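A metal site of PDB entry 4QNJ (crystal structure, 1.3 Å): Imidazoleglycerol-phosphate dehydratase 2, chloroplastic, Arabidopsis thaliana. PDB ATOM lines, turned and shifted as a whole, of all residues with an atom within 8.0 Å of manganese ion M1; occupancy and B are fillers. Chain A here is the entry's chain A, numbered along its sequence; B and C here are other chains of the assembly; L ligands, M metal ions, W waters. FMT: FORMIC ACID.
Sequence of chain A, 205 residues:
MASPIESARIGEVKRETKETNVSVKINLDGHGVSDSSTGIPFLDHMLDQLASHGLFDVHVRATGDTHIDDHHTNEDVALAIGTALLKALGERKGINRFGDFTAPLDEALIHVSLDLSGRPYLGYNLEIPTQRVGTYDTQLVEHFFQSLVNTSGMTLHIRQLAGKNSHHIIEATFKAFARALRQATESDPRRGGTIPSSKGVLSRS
The side-chain carboxylate of Glu 107 of chain B sits at hydrogen-bond distance from a ring nitrogen (ND1) of His 168 of chain B, 2.8 Å away. The side-chain amide oxygen (OD1) of Asn 165 of chain B sits at hydrogen-bond distance from the backbone NH (N) of His 168 of chain B (3.0 Å). ND1 of His 143 is in hydrogen-bond range of OG of Ser 147 (3.0 Å).
Water W1 lies within hydrogen-bond range of the side-chain carboxylate of Asp 106 of chain B (2.7 Å), the side-chain carboxylate of Glu 75 (2.7 Å) and the guanidinium group of Arg 119 of chain C (3.4 Å).
Manganese ion M1 is bound by water W1 (2.2 Å), an oxygen (O2) of the ligand (2.2 Å), a ring nitrogen (NE2) of His 71 (2.3 Å), the side-chain carboxylate of Glu 75 (2.3 Å), a ring nitrogen (NE2) of His 168 of chain B (2.3 Å) and a ring nitrogen (NE2) of His 143 (2.3 Å).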
ATOM      1  N   HIS A  71     -35.445   7.503 -25.164  1.00  0.00           N
ATOM      2  CA  HIS A  71     -34.081   6.995 -24.978  1.00  0.00           C
ATOM      3  C   HIS A  71     -32.987   8.045 -25.200  1.00  0.00           C
ATOM      4  O   HIS A  71     -32.104   8.227 -24.352  1.00  0.00           O
ATOM      5  CB  HIS A  71     -33.838   5.833 -25.926  1.00  0.00           C
ATOM      6  CG  HIS A  71     -32.547   5.096 -25.701  1.00  0.00           C
ATOM      7  ND1 HIS A  71     -32.522   3.744 -25.434  1.00  0.00           N
ATOM      8  CD2 HIS A  71     -31.244   5.486 -25.749  1.00  0.00           C
ATOM      9  CE1 HIS A  71     -31.279   3.336 -25.313  1.00  0.00           C
ATOM     10  NE2 HIS A  71     -30.482   4.369 -25.498  1.00  0.00           N
ATOM     11  N   HIS A  72     -33.002   8.706 -26.352  1.00  0.00           N
ATOM     12  CA  HIS A  72     -31.881   9.618 -26.664  1.00  0.00           C
ATOM     13  C   HIS A  72     -31.833  10.802 -25.680  1.00  0.00           C
ATOM     14  O   HIS A  72     -30.762  11.189 -25.216  1.00  0.00           O
ATOM     15  CB  HIS A  72     -31.928  10.129 -28.114  1.00  0.00           C
ATOM     16  CG  HIS A  72     -31.880   9.066 -29.172  1.00  0.00           C
ATOM     17  ND1 HIS A  72     -32.421   9.276 -30.424  1.00  0.00           N
ATOM     18  CD2 HIS A  72     -31.387   7.798 -29.199  1.00  0.00           C
ATOM     19  CE1 HIS A  72     -32.257   8.203 -31.181  1.00  0.00           C
ATOM     20  NE2 HIS A  72     -31.623   7.291 -30.454  1.00  0.00           N
ATOM     21  N   ASN A  74     -33.041  10.837 -22.576  1.00  0.00           N
ATOM     22  CA  ASN A  74     -32.666  10.306 -21.262  1.00  0.00           C
ATOM     23  C   ASN A  74     -31.154  10.146 -21.171  1.00  0.00           C
ATOM     24  O   ASN A  74     -30.527  10.553 -20.228  1.00  0.00           O
ATOM     25  CB  ASN A  74     -33.395   8.966 -21.083  1.00  0.00           C
ATOM     26  CG  ASN A  74     -33.146   8.311 -19.731  1.00  0.00           C
ATOM     27  OD1 ASN A  74     -33.785   8.646 -18.750  1.00  0.00           O
ATOM     28  ND2 ASN A  74     -32.270   7.345 -19.700  1.00  0.00           N
ATOM     29  N   GLU A  75     -30.592   9.551 -22.221  1.00  0.00           N
ATOM     30  CA  GLU A  75     -29.141   9.295 -22.291  1.00  0.00           C
ATOM     31  C   GLU A  75     -28.342  10.599 -22.307  1.00  0.00           C
ATOM     32  O   GLU A  75     -27.380  10.785 -21.553  1.00  0.00           O
ATOM     33  CB  GLU A  75     -28.834   8.445 -23.519  1.00  0.00           C
ATOM     34  CG  GLU A  75     -27.344   8.223 -23.742  1.00  0.00           C
ATOM     35  CD  GLU A  75     -27.007   7.097 -24.716  1.00  0.00           C
ATOM     36  OE1 GLU A  75     -27.948   6.509 -25.296  1.00  0.00           O
ATOM     37  OE2 GLU A  75     -25.799   6.817 -24.876  1.00  0.00           O
ATOM     38  N   ASP A  76     -28.760  11.531 -23.161  1.00  0.00           N
ATOM     39  CA  ASP A  76     -27.992  12.770 -23.343  1.00  0.00           C
ATOM     40  C   ASP A  76     -28.088  13.683 -22.097  1.00  0.00           C
ATOM     41  O   ASP A  76     -27.125  14.356 -21.732  1.00  0.00           O
ATOM     42  CB  ASP A  76     -28.401  13.493 -24.628  1.00  0.00           C
ATOM     43  CG  ASP A  76     -27.926  12.767 -25.876  1.00  0.00           C
ATOM     44  OD1 ASP A  76     -27.052  11.877 -25.763  1.00  0.00           O
ATOM     45  OD2 ASP A  76     -28.424  13.062 -26.977  1.00  0.00           O
ATOM     46  N   LEU A  79     -25.683  11.906 -19.568  1.00  0.00           N
ATOM     47  CA  LEU A  79     -24.285  12.181 -19.945  1.00  0.00           C
ATOM     48  C   LEU A  79     -23.878  13.595 -19.503  1.00  0.00           C
ATOM     49  O   LEU A  79     -22.814  13.820 -18.923  1.00  0.00           O
ATOM     50  CB  LEU A  79     -24.080  12.037 -21.450  1.00  0.00           C
ATOM     51  CG  LEU A  79     -24.164  10.614 -22.022  1.00  0.00           C
ATOM     52  CD1 LEU A  79     -24.209  10.638 -23.529  1.00  0.00           C
ATOM     53  CD2 LEU A  79     -23.023   9.731 -21.532  1.00  0.00           C
ATOM     54  N   LEU A 140     -34.978   2.625 -18.949  1.00  0.00           N
ATOM     55  CA  LEU A 140     -34.178   3.855 -19.037  1.00  0.00           C
ATOM     56  C   LEU A 140     -33.560   4.284 -17.709  1.00  0.00           C
ATOM     57  O   LEU A 140     -32.644   5.097 -17.696  1.00  0.00           O
ATOM     58  CB  LEU A 140     -35.006   4.973 -19.662  1.00  0.00           C
ATOM     59  CG  LEU A 140     -35.445   4.679 -21.108  1.00  0.00           C
ATOM     60  CD1 LEU A 140     -36.257   5.832 -21.688  1.00  0.00           C
ATOM     61  CD2 LEU A 140     -34.289   4.309 -22.037  1.00  0.00           C
ATOM     62  N   HIS A 143     -30.060   2.988 -17.777  1.00  0.00           N
ATOM     63  CA  HIS A 143     -29.263   3.722 -18.762  1.00  0.00           C
ATOM     64  C   HIS A 143     -28.931   5.126 -18.245  1.00  0.00           C
ATOM     65  O   HIS A 143     -27.848   5.664 -18.519  1.00  0.00           O
ATOM     66  CB  HIS A 143     -30.006   3.826 -20.092  1.00  0.00           C
ATOM     67  CG  HIS A 143     -29.116   4.057 -21.293  1.00  0.00           C
ATOM     68  ND1 HIS A 143     -27.985   4.843 -21.265  1.00  0.00           N
ATOM     69  CD2 HIS A 143     -29.219   3.595 -22.560  1.00  0.00           C
ATOM     70  CE1 HIS A 143     -27.442   4.862 -22.472  1.00  0.00           C
ATOM     71  NE2 HIS A 143     -28.167   4.111 -23.269  1.00  0.00           N
ATOM     72  N   SER A 147     -24.959   6.097 -17.962  1.00  0.00           N
ATOM     73  CA  SER A 147     -24.440   7.229 -18.709  1.00  0.00           C
ATOM     74  C   SER A 147     -23.835   8.293 -17.778  1.00  0.00           C
ATOM     75  O   SER A 147     -22.752   8.828 -18.030  1.00  0.00           O
ATOM     76  CB  SER A 147     -25.541   7.820 -19.578  1.00  0.00           C
ATOM     77  OG  SER A 147     -25.900   6.941 -20.619  1.00  0.00           O
ATOM     78  N   LEU B 105     -23.840  -2.298 -29.970  1.00  0.00           N
ATOM     79  CA  LEU B 105     -24.306  -0.995 -29.501  1.00  0.00           C
ATOM     80  C   LEU B 105     -24.307  -1.149 -27.993  1.00  0.00           C
ATOM     81  O   LEU B 105     -25.170  -1.795 -27.421  1.00  0.00           O
ATOM     82  CB  LEU B 105     -25.689  -0.583 -30.034  1.00  0.00           C
ATOM     83  CG  LEU B 105     -25.987   0.934 -29.848  1.00  0.00           C
ATOM     84  CD1 LEU B 105     -27.360   1.319 -30.370  1.00  0.00           C
ATOM     85  CD2 LEU B 105     -25.776   1.486 -28.452  1.00  0.00           C
ATOM     86  N   ASP B 106     -23.276  -0.602 -27.373  1.00  0.00           N
ATOM     87  CA  ASP B 106     -23.067  -0.760 -25.931  1.00  0.00           C
ATOM     88  C   ASP B 106     -23.096  -2.264 -25.562  1.00  0.00           C
ATOM     89  O   ASP B 106     -22.291  -3.023 -26.100  1.00  0.00           O
ATOM     90  CB  ASP B 106     -24.016   0.107 -25.092  1.00  0.00           C
ATOM     91  CG  ASP B 106     -23.826   1.590 -25.318  1.00  0.00           C
ATOM     92  OD1 ASP B 106     -22.838   2.015 -25.967  1.00  0.00           O
ATOM     93  OD2 ASP B 106     -24.658   2.336 -24.760  1.00  0.00           O
ATOM     94  N   GLU B 107     -24.017  -2.669 -24.694  1.00  0.00           N
ATOM     95  CA  GLU B 107     -24.067  -4.076 -24.232  1.00  0.00           C
ATOM     96  C   GLU B 107     -24.653  -5.038 -25.267  1.00  0.00           C
ATOM     97  O   GLU B 107     -24.527  -6.249 -25.113  1.00  0.00           O
ATOM     98  CB  GLU B 107     -24.860  -4.160 -22.922  1.00  0.00           C
ATOM     99  CG  GLU B 107     -26.373  -4.378 -23.020  1.00  0.00           C
ATOM    100  CD  GLU B 107     -27.154  -3.331 -23.784  1.00  0.00           C
ATOM    101  OE1 GLU B 107     -26.708  -2.183 -23.890  1.00  0.00           O
ATOM    102  OE2 GLU B 107     -28.268  -3.689 -24.246  1.00  0.00           O
ATOM    103  N   ASN B 165     -31.022  -3.784 -23.415  1.00  0.00           N
ATOM    104  CA  ASN B 165     -31.882  -2.653 -23.742  1.00  0.00           C
ATOM    105  C   ASN B 165     -32.511  -2.887 -25.113  1.00  0.00           C
ATOM    106  O   ASN B 165     -31.802  -3.156 -26.081  1.00  0.00           O
ATOM    107  CB  ASN B 165     -31.077  -1.370 -23.729  1.00  0.00           C
ATOM    108  CG  ASN B 165     -31.932  -0.167 -24.077  1.00  0.00           C
ATOM    109  OD1 ASN B 165     -32.220   0.070 -25.239  1.00  0.00           O
ATOM    110  ND2 ASN B 165     -32.355   0.570 -23.058  1.00  0.00           N
ATOM    111  N   HIS B 167     -34.009  -0.962 -27.375  1.00  0.00           N
ATOM    112  CA  HIS B 167     -33.571  -0.020 -28.417  1.00  0.00           C
ATOM    113  C   HIS B 167     -32.161  -0.390 -28.884  1.00  0.00           C
ATOM    114  O   HIS B 167     -31.891  -0.414 -30.085  1.00  0.00           O
ATOM    115  CB  HIS B 167     -33.698   1.391 -27.847  1.00  0.00           C
ATOM    116  CG  HIS B 167     -33.400   2.539 -28.778  1.00  0.00           C
ATOM    117  ND1 HIS B 167     -34.125   3.707 -28.698  1.00  0.00           N
ATOM    118  CD2 HIS B 167     -32.403   2.783 -29.666  1.00  0.00           C
ATOM    119  CE1 HIS B 167     -33.600   4.615 -29.500  1.00  0.00           C
ATOM    120  NE2 HIS B 167     -32.565   4.070 -30.118  1.00  0.00           N
ATOM    121  N   HIS B 168     -31.272  -0.696 -27.954  1.00  0.00           N
ATOM    122  CA  HIS B 168     -29.918  -1.126 -28.348  1.00  0.00           C
ATOM    123  C   HIS B 168     -29.904  -2.403 -29.194  1.00  0.00           C
ATOM    124  O   HIS B 168     -29.197  -2.500 -30.186  1.00  0.00           O
ATOM    125  CB  HIS B 168     -29.020  -1.332 -27.139  1.00  0.00           C
ATOM    126  CG  HIS B 168     -28.666  -0.064 -26.436  1.00  0.00           C
ATOM    127  ND1 HIS B 168     -27.959  -0.057 -25.255  1.00  0.00           N
ATOM    128  CD2 HIS B 168     -28.929   1.239 -26.719  1.00  0.00           C
ATOM    129  CE1 HIS B 168     -27.776   1.196 -24.866  1.00  0.00           C
ATOM    130  NE2 HIS B 168     -28.356   1.993 -25.737  1.00  0.00           N
ATOM    131  N   GLU B 171     -31.415  -1.523 -32.702  1.00  0.00           N
ATOM    132  CA  GLU B 171     -30.527  -0.616 -33.448  1.00  0.00           C
ATOM    133  C   GLU B 171     -29.231  -1.329 -33.870  1.00  0.00           C
ATOM    134  O   GLU B 171     -28.774  -1.182 -35.016  1.00  0.00           O
ATOM    135  CB  GLU B 171     -30.254   0.650 -32.642  1.00  0.00           C
ATOM    136  CG  GLU B 171     -29.457   1.683 -33.414  1.00  0.00           C
ATOM    137  CD  GLU B 171     -29.391   3.028 -32.734  1.00  0.00           C
ATOM    138  OE1 GLU B 171     -30.344   3.407 -32.038  1.00  0.00           O
ATOM    139  OE2 GLU B 171     -28.344   3.697 -32.897  1.00  0.00           O
ATOM    140  N   ARG C 119     -18.295   5.659 -25.934  1.00  0.00           N
ATOM    141  CA  ARG C 119     -19.011   5.156 -24.753  1.00  0.00           C
ATOM    142  C   ARG C 119     -18.305   3.899 -24.255  1.00  0.00           C
ATOM    143  O   ARG C 119     -18.289   2.898 -24.976  1.00  0.00           O
ATOM    144  CB  ARG C 119     -20.456   4.825 -25.091  1.00  0.00           C
ATOM    145  CG  ARG C 119     -21.272   6.006 -25.595  1.00  0.00           C
ATOM    146  CD  ARG C 119     -22.731   5.620 -25.854  1.00  0.00           C
ATOM    147  NE  ARG C 119     -22.777   4.633 -26.921  1.00  0.00           N
ATOM    148  CZ  ARG C 119     -22.748   4.878 -28.220  1.00  0.00           C
ATOM    149  NH1 ARG C 119     -22.810   6.130 -28.653  1.00  0.00           N
ATOM    150  NH2 ARG C 119     -22.697   3.891 -29.088  1.00  0.00           N
HETATM  151  C   FMT L   1     -29.504   4.608 -28.551  1.00  0.00           C
HETATM  152  O1  FMT L   1     -29.466   5.131 -29.670  1.00  0.00           O
HETATM  153  O2  FMT L   1     -28.452   4.643 -27.774  1.00  0.00           O
HETATM  154 MN    MN M   1     -28.220   4.274 -25.611  1.00  0.00          MN
HETATM  155 MN    MN M   2     -30.995   5.273 -31.283  1.00  0.00          MN
HETATM  156  O   HOH W   1     -26.066   4.320 -25.959  1.00  0.00           O
